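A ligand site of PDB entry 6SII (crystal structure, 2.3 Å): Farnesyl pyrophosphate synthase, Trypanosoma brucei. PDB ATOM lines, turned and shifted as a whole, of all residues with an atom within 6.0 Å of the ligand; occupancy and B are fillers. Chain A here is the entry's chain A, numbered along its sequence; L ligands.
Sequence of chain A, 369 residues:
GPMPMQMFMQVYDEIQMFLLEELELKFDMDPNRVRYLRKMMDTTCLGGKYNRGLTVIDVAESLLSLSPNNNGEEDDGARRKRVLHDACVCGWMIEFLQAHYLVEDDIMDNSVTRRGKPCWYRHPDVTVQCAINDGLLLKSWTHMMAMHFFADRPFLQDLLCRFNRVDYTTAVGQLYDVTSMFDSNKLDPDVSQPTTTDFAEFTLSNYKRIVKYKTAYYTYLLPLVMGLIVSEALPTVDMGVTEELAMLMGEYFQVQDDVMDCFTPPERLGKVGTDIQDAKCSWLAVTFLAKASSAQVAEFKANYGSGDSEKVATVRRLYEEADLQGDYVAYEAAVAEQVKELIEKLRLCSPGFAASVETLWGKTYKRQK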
ATOM      1  N   ASP A 177     -28.191  14.289  -6.882  1.00  0.00           N
ATOM      2  CA  ASP A 177     -27.175  15.108  -6.226  1.00  0.00           C
ATOM      3  C   ASP A 177     -26.204  15.755  -7.202  1.00  0.00           C
ATOM      4  O   ASP A 177     -25.933  16.944  -7.105  1.00  0.00           O
ATOM      5  CB  ASP A 177     -26.414  14.269  -5.195  1.00  0.00           C
ATOM      6  CG  ASP A 177     -25.459  15.072  -4.344  1.00  0.00           C
ATOM      7  OD1 ASP A 177     -25.912  16.091  -3.748  1.00  0.00           O
ATOM      8  OD2 ASP A 177     -24.266  14.708  -4.276  1.00  0.00           O
ATOM      9  N   TYR A 207     -34.181  18.915  -1.725  1.00  0.00           N
ATOM     10  CA  TYR A 207     -33.107  18.608  -0.799  1.00  0.00           C
ATOM     11  C   TYR A 207     -33.449  17.258  -0.131  1.00  0.00           C
ATOM     12  O   TYR A 207     -32.600  16.370  -0.064  1.00  0.00           O
ATOM     13  CB  TYR A 207     -32.976  19.753   0.261  1.00  0.00           C
ATOM     14  CG  TYR A 207     -31.974  19.459   1.354  1.00  0.00           C
ATOM     15  CD1 TYR A 207     -30.607  19.452   1.090  1.00  0.00           C
ATOM     16  CD2 TYR A 207     -32.396  19.094   2.626  1.00  0.00           C
ATOM     17  CE1 TYR A 207     -29.678  19.115   2.072  1.00  0.00           C
ATOM     18  CE2 TYR A 207     -31.480  18.715   3.612  1.00  0.00           C
ATOM     19  CZ  TYR A 207     -30.127  18.743   3.332  1.00  0.00           C
ATOM     20  OH  TYR A 207     -29.216  18.414   4.288  1.00  0.00           O
ATOM     21  N   ILE A 210     -32.973  14.230  -2.450  1.00  0.00           N
ATOM     22  CA  ILE A 210     -31.573  13.861  -2.536  1.00  0.00           C
ATOM     23  C   ILE A 210     -31.213  13.061  -1.287  1.00  0.00           C
ATOM     24  O   ILE A 210     -30.715  11.968  -1.409  1.00  0.00           O
ATOM     25  CB  ILE A 210     -30.625  15.082  -2.729  1.00  0.00           C
ATOM     26  CG1 ILE A 210     -30.930  15.841  -4.032  1.00  0.00           C
ATOM     27  CG2 ILE A 210     -29.152  14.621  -2.683  1.00  0.00           C
ATOM     28  CD1 ILE A 210     -30.312  17.244  -4.173  1.00  0.00           C
ATOM     29  N   VAL A 211     -31.517  13.595  -0.109  1.00  0.00           N
ATOM     30  CA  VAL A 211     -31.203  12.950   1.180  1.00  0.00           C
ATOM     31  C   VAL A 211     -31.799  11.533   1.260  1.00  0.00           C
ATOM     32  O   VAL A 211     -31.074  10.600   1.556  1.00  0.00           O
ATOM     33  CB  VAL A 211     -31.587  13.866   2.392  1.00  0.00           C
ATOM     34  CG1 VAL A 211     -31.279  13.185   3.726  1.00  0.00           C
ATOM     35  CG2 VAL A 211     -30.854  15.199   2.314  1.00  0.00           C
ATOM     36  N   LYS A 214     -30.019   9.315  -1.894  1.00  0.00           N
ATOM     37  CA  LYS A 214     -28.562   9.277  -1.764  1.00  0.00           C
ATOM     38  C   LYS A 214     -28.064   8.696  -0.448  1.00  0.00           C
ATOM     39  O   LYS A 214     -27.068   7.951  -0.468  1.00  0.00           O
ATOM     40  CB  LYS A 214     -27.975  10.681  -1.947  1.00  0.00           C
ATOM     41  CG  LYS A 214     -26.482  10.702  -2.119  1.00  0.00           C
ATOM     42  CD  LYS A 214     -25.891  12.075  -2.015  1.00  0.00           C
ATOM     43  CE  LYS A 214     -24.390  12.026  -2.245  1.00  0.00           C
ATOM     44  NZ  LYS A 214     -24.027  11.883  -3.679  1.00  0.00           N
ATOM     45  N   THR A 215     -28.705   9.067   0.697  1.00  0.00           N
ATOM     46  CA  THR A 215     -28.162   8.614   1.975  1.00  0.00           C
ATOM     47  C   THR A 215     -29.131   7.818   2.895  1.00  0.00           C
ATOM     48  O   THR A 215     -28.707   6.776   3.412  1.00  0.00           O
ATOM     49  CB  THR A 215     -27.518   9.777   2.753  1.00  0.00           C
ATOM     50  OG1 THR A 215     -28.430  10.840   2.979  1.00  0.00           O
ATOM     51  CG2 THR A 215     -26.287  10.346   2.042  1.00  0.00           C
ATOM     52  N   GLN A 254     -28.042  14.843   7.704  1.00  0.00           N
ATOM     53  CA  GLN A 254     -27.566  15.610   6.564  1.00  0.00           C
ATOM     54  C   GLN A 254     -27.482  17.107   6.809  1.00  0.00           C
ATOM     55  O   GLN A 254     -26.539  17.744   6.336  1.00  0.00           O
ATOM     56  CB  GLN A 254     -28.362  15.313   5.282  1.00  0.00           C
ATOM     57  CG  GLN A 254     -27.554  15.601   4.012  1.00  0.00           C
ATOM     58  CD  GLN A 254     -26.187  14.948   4.033  1.00  0.00           C
ATOM     59  OE1 GLN A 254     -26.071  13.725   4.099  1.00  0.00           O
ATOM     60  NE2 GLN A 254     -25.117  15.737   4.016  1.00  0.00           N
ATOM     61  N   ASP A 257     -24.481  17.583   8.975  1.00  0.00           N
ATOM     62  CA  ASP A 257     -23.324  17.339   8.116  1.00  0.00           C
ATOM     63  C   ASP A 257     -23.008  18.493   7.178  1.00  0.00           C
ATOM     64  O   ASP A 257     -21.824  18.782   6.954  1.00  0.00           O
ATOM     65  CB  ASP A 257     -23.559  16.086   7.277  1.00  0.00           C
ATOM     66  CG  ASP A 257     -22.689  14.913   7.634  1.00  0.00           C
ATOM     67  OD1 ASP A 257     -22.158  14.885   8.769  1.00  0.00           O
ATOM     68  OD2 ASP A 257     -22.556  14.008   6.796  1.00  0.00           O
ATOM     69  N   ASP A 258     -24.068  19.116   6.591  1.00  0.00           N
ATOM     70  CA  ASP A 258     -23.998  20.248   5.662  1.00  0.00           C
ATOM     71  C   ASP A 258     -23.489  21.482   6.364  1.00  0.00           C
ATOM     72  O   ASP A 258     -22.713  22.232   5.773  1.00  0.00           O
ATOM     73  CB  ASP A 258     -25.375  20.544   5.032  1.00  0.00           C
ATOM     74  CG  ASP A 258     -25.846  19.539   3.996  1.00  0.00           C
ATOM     75  OD1 ASP A 258     -25.099  18.604   3.695  1.00  0.00           O
ATOM     76  OD2 ASP A 258     -26.969  19.687   3.494  1.00  0.00           O
ATOM     77  N   MET A 260     -21.706  21.516   9.237  1.00  0.00           N
ATOM     78  CA  MET A 260     -20.316  21.228   9.605  1.00  0.00           C
ATOM     79  C   MET A 260     -19.382  21.340   8.404  1.00  0.00           C
ATOM     80  O   MET A 260     -18.236  21.768   8.559  1.00  0.00           O
ATOM     81  CB  MET A 260     -20.213  19.817  10.188  1.00  0.00           C
ATOM     82  CG  MET A 260     -20.691  19.684  11.611  1.00  0.00           C
ATOM     83  SD  MET A 260     -20.514  17.935  12.068  1.00  0.00           S
ATOM     84  CE  MET A 260     -18.788  17.936  12.705  1.00  0.00           C
ATOM     85  N   ASP A 261     -19.859  20.973   7.204  1.00  0.00           N
ATOM     86  CA  ASP A 261     -19.093  21.070   5.960  1.00  0.00           C
ATOM     87  C   ASP A 261     -18.671  22.530   5.701  1.00  0.00           C
ATOM     88  O   ASP A 261     -17.588  22.765   5.172  1.00  0.00           O
ATOM     89  CB  ASP A 261     -19.916  20.524   4.782  1.00  0.00           C
ATOM     90  CG  ASP A 261     -19.143  20.374   3.492  1.00  0.00           C
ATOM     91  OD1 ASP A 261     -18.923  21.399   2.815  1.00  0.00           O
ATOM     92  OD2 ASP A 261     -18.773  19.240   3.151  1.00  0.00           O
ATOM     93  N   THR A 264     -17.335  23.921  10.327  1.00  0.00           N
ATOM     94  CA  THR A 264     -16.362  23.176  11.139  1.00  0.00           C
ATOM     95  C   THR A 264     -14.949  23.454  10.603  1.00  0.00           C
ATOM     96  O   THR A 264     -14.706  23.160   9.428  1.00  0.00           O
ATOM     97  CB  THR A 264     -16.783  21.696  11.258  1.00  0.00           C
ATOM     98  OG1 THR A 264     -17.968  21.629  12.041  1.00  0.00           O
ATOM     99  CG2 THR A 264     -15.712  20.818  11.872  1.00  0.00           C
ATOM    100  N   LEU A 269     -10.836  20.669  13.385  1.00  0.00           N
ATOM    101  CA  LEU A 269     -11.985  19.898  13.892  1.00  0.00           C
ATOM    102  C   LEU A 269     -12.596  18.899  12.867  1.00  0.00           C
ATOM    103  O   LEU A 269     -13.715  18.426  13.098  1.00  0.00           O
ATOM    104  CB  LEU A 269     -13.059  20.858  14.447  1.00  0.00           C
ATOM    105  CG  LEU A 269     -13.322  20.838  15.959  1.00  0.00           C
ATOM    106  CD1 LEU A 269     -13.836  22.183  16.442  1.00  0.00           C
ATOM    107  CD2 LEU A 269     -14.285  19.715  16.351  1.00  0.00           C
ATOM    108  N   GLY A 270     -11.877  18.563  11.788  1.00  0.00           N
ATOM    109  CA  GLY A 270     -12.397  17.607  10.803  1.00  0.00           C
ATOM    110  C   GLY A 270     -11.613  17.302   9.540  1.00  0.00           C
ATOM    111  O   GLY A 270     -10.426  16.938   9.588  1.00  0.00           O
ATOM    112  N   LYS A 271     -12.334  17.371   8.381  1.00  0.00           N
ATOM    113  CA  LYS A 271     -11.856  17.129   7.010  1.00  0.00           C
ATOM    114  C   LYS A 271     -12.096  18.359   6.103  1.00  0.00           C
ATOM    115  O   LYS A 271     -12.432  19.435   6.612  1.00  0.00           O
ATOM    116  CB  LYS A 271     -12.479  15.844   6.425  1.00  0.00           C
ATOM    117  CG  LYS A 271     -11.601  14.615   6.683  1.00  0.00           C
ATOM    118  CD  LYS A 271     -12.094  13.382   5.943  1.00  0.00           C
ATOM    119  CE  LYS A 271     -11.203  12.174   6.174  1.00  0.00           C
ATOM    120  NZ  LYS A 271     -11.683  10.983   5.429  1.00  0.00           N
ATOM    121  N   VAL A 272     -11.868  18.235   4.774  1.00  0.00           N
ATOM    122  CA  VAL A 272     -12.041  19.373   3.862  1.00  0.00           C
ATOM    123  C   VAL A 272     -13.496  19.477   3.401  1.00  0.00           C
ATOM    124  O   VAL A 272     -14.033  18.525   2.829  1.00  0.00           O
ATOM    125  CB  VAL A 272     -11.047  19.414   2.660  1.00  0.00           C
ATOM    126  CG1 VAL A 272     -10.820  20.854   2.186  1.00  0.00           C
ATOM    127  CG2 VAL A 272      -9.719  18.738   2.995  1.00  0.00           C
ATOM    128  N   GLY A 273     -14.114  20.625   3.686  1.00  0.00           N
ATOM    129  CA  GLY A 273     -15.479  20.948   3.287  1.00  0.00           C
ATOM    130  C   GLY A 273     -15.470  21.708   1.973  1.00  0.00           C
ATOM    131  O   GLY A 273     -14.843  22.765   1.869  1.00  0.00           O
ATOM    132  N   THR A 274     -16.166  21.155   0.950  1.00  0.00           N
ATOM    133  CA  THR A 274     -16.191  21.723  -0.396  1.00  0.00           C
ATOM    134  C   THR A 274     -17.587  21.963  -0.997  1.00  0.00           C
ATOM    135  O   THR A 274     -17.667  22.241  -2.195  1.00  0.00           O
ATOM    136  CB  THR A 274     -15.390  20.807  -1.349  1.00  0.00           C
ATOM    137  OG1 THR A 274     -15.807  19.447  -1.156  1.00  0.00           O
ATOM    138  CG2 THR A 274     -13.888  20.989  -1.235  1.00  0.00           C
ATOM    139  N   ASP A 275     -18.667  21.861  -0.201  1.00  0.00           N
ATOM    140  CA  ASP A 275     -20.038  22.051  -0.716  1.00  0.00           C
ATOM    141  C   ASP A 275     -20.221  23.371  -1.451  1.00  0.00           C
ATOM    142  O   ASP A 275     -20.856  23.384  -2.504  1.00  0.00           O
ATOM    143  CB  ASP A 275     -21.111  21.862   0.377  1.00  0.00           C
ATOM    144  CG  ASP A 275     -21.399  20.422   0.767  1.00  0.00           C
ATOM    145  OD1 ASP A 275     -21.085  19.517  -0.033  1.00  0.00           O
ATOM    146  OD2 ASP A 275     -21.959  20.207   1.856  1.00  0.00           O
ATOM    147  N   LYS A 280     -23.132  22.504  -4.221  1.00  0.00           N
ATOM    148  CA  LYS A 280     -24.073  21.500  -3.751  1.00  0.00           C
ATOM    149  C   LYS A 280     -25.387  22.086  -3.258  1.00  0.00           C
ATOM    150  O   LYS A 280     -25.439  23.213  -2.738  1.00  0.00           O
ATOM    151  CB  LYS A 280     -23.433  20.610  -2.663  1.00  0.00           C
ATOM    152  CG  LYS A 280     -22.312  19.728  -3.192  1.00  0.00           C
ATOM    153  CD  LYS A 280     -22.845  18.558  -4.055  1.00  0.00           C
ATOM    154  CE  LYS A 280     -21.930  18.125  -5.177  1.00  0.00           C
ATOM    155  NZ  LYS A 280     -22.621  17.246  -6.150  1.00  0.00           N
ATOM    156  N   CYS A 281     -26.456  21.312  -3.433  1.00  0.00           N
ATOM    157  CA  CYS A 281     -27.779  21.657  -2.970  1.00  0.00           C
ATOM    158  C   CYS A 281     -27.786  21.306  -1.482  1.00  0.00           C
ATOM    159  O   CYS A 281     -28.352  20.297  -1.080  1.00  0.00           O
ATOM    160  CB  CYS A 281     -28.836  20.888  -3.749  1.00  0.00           C
ATOM    161  SG  CYS A 281     -30.539  21.232  -3.248  1.00  0.00           S
ATOM    162  N   SER A 282     -27.119  22.144  -0.650  1.00  0.00           N
ATOM    163  CA  SER A 282     -27.043  21.928   0.797  1.00  0.00           C
ATOM    164  C   SER A 282     -28.205  22.597   1.532  1.00  0.00           C
ATOM    165  O   SER A 282     -28.842  23.490   0.988  1.00  0.00           O
ATOM    166  CB  SER A 282     -25.705  22.424   1.339  1.00  0.00           C
ATOM    167  OG  SER A 282     -25.684  23.815   1.596  1.00  0.00           O
ATOM    168  N   TRP A 283     -28.460  22.169   2.782  1.00  0.00           N
ATOM    169  CA  TRP A 283     -29.492  22.725   3.618  1.00  0.00           C
ATOM    170  C   TRP A 283     -29.247  24.209   3.812  1.00  0.00           C
ATOM    171  O   TRP A 283     -30.196  24.976   3.815  1.00  0.00           O
ATOM    172  CB  TRP A 283     -29.570  22.014   4.970  1.00  0.00           C
ATOM    173  CG  TRP A 283     -30.645  22.597   5.854  1.00  0.00           C
ATOM    174  CD1 TRP A 283     -31.957  22.253   5.859  1.00  0.00           C
ATOM    175  CD2 TRP A 283     -30.514  23.708   6.774  1.00  0.00           C
ATOM    176  NE1 TRP A 283     -32.634  22.993   6.796  1.00  0.00           N
ATOM    177  CE2 TRP A 283     -31.777  23.890   7.374  1.00  0.00           C
ATOM    178  CE3 TRP A 283     -29.429  24.501   7.211  1.00  0.00           C
ATOM    179  CZ2 TRP A 283     -32.022  24.914   8.298  1.00  0.00           C
ATOM    180  CZ3 TRP A 283     -29.653  25.475   8.169  1.00  0.00           C
ATOM    181  CH2 TRP A 283     -30.949  25.700   8.686  1.00  0.00           C
HETATM  182  C1  LIG L   1     -17.236  18.010   9.428  1.00  0.00           C
HETATM  183  C2  LIG L   1     -18.218  17.031   9.336  1.00  0.00           C
HETATM  184  C3  LIG L   1     -18.606  16.516   8.111  1.00  0.00           C
HETATM  185  C4  LIG L   1     -20.768  16.110   1.773  1.00  0.00           C
HETATM  186  C5  LIG L   1     -19.554  16.405   2.661  1.00  0.00           C
HETATM  187  C6  LIG L   1     -21.369  16.351   4.272  1.00  0.00           C
HETATM  188  C7  LIG L   1     -22.223  17.294   3.416  1.00  0.00           C
HETATM  189  C8  LIG L   1     -21.835  17.173   1.951  1.00  0.00           C
HETATM  190  C9  LIG L   1     -23.663  17.603   0.338  1.00  0.00           C
HETATM  191  C10 LIG L   1     -25.076  17.111   0.135  1.00  0.00           C
HETATM  192  C11 LIG L   1     -26.065  17.952  -0.361  1.00  0.00           C
HETATM  193  C12 LIG L   1     -27.391  17.531  -0.414  1.00  0.00           C
HETATM  194  C13 LIG L   1     -27.746  16.267   0.023  1.00  0.00           C
HETATM  195  C14 LIG L   1     -26.752  15.419   0.474  1.00  0.00           C
HETATM  196  C15 LIG L   1     -25.431  15.820   0.530  1.00  0.00           C
HETATM  197  C16 LIG L   1     -17.986  16.972   6.947  1.00  0.00           C
HETATM  198  C17 LIG L   1     -16.977  17.958   7.050  1.00  0.00           C
HETATM  199  C18 LIG L   1     -16.599  18.488   8.290  1.00  0.00           C
HETATM  200  C19 LIG L   1     -18.091  16.643   5.551  1.00  0.00           C
HETATM  201  C20 LIG L   1     -17.156  17.394   4.900  1.00  0.00           C
HETATM  202  N1  LIG L   1     -16.488  18.196   5.795  1.00  0.00           N
HETATM  203  C21 LIG L   1     -19.120  15.739   4.942  1.00  0.00           C
HETATM  204  N2  LIG L   1     -19.934  16.598   4.069  1.00  0.00           N
HETATM  205  N3  LIG L   1     -22.845  16.610   1.037  1.00  0.00           N
HETATM  206 CL1  LIG L   1     -27.157  13.794   0.950  1.00  0.00          CL
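N of Asp 275 lies within hydrogen-bond range of OD1 of Asp 261. O of Asp 275 is in hydrogen-bond range of N of Lys 280, 3.0 Å away. The side-chain carboxylate (OD1) of Asp 258 is in hydrogen-bond range of the side-chain amide nitrogen (NE2) of Gln 254, 2.9 Å away. OH of Tyr 207 lies within hydrogen-bond range of OD2 of Asp 258 (2.7 Å). N of Trp 283 is in hydrogen-bond range of OD2 of Asp 258 (3.0 Å). O of Gln 254 lies close to OH of Tyr 207. The side-chain amino group (NZ) of Lys 214 lies within salt-bridge range of the side-chain carboxylate (OD2) of Asp 177, 2.9 Å away. The side-chain hydroxyl of Thr 215 sits at hydrogen-bond distance from the backbone carbonyl oxygen of Val 211, 3.0 Å away.
The side-chain carboxylate (OD2) of Asp 261 is in salt-bridge range of a nitrogen (N2) of the ligand, at 3.0 Å. OD1 of Asp 275 is in salt-bridge range of N3 of the ligand, 3.6 Å away.
Merely in contact with the ligand: Cys 281 (3.0 Å), Asp 258 (3.2 Å), Gln 254 (3.3 Å), Ile 210 (3.5 Å), Met 260 (3.5 Å), Asp 257 (3.6 Å), Lys 214 (3.7 Å), Thr 215 (3.7 Å), Tyr 207 (3.7 Å), Gly 273 (3.9 Å), Val 272 (3.9 Å) and Asp 177 (3.9 Å). Of the 23 residues printed, 14 come within 4 Å of the ligand.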
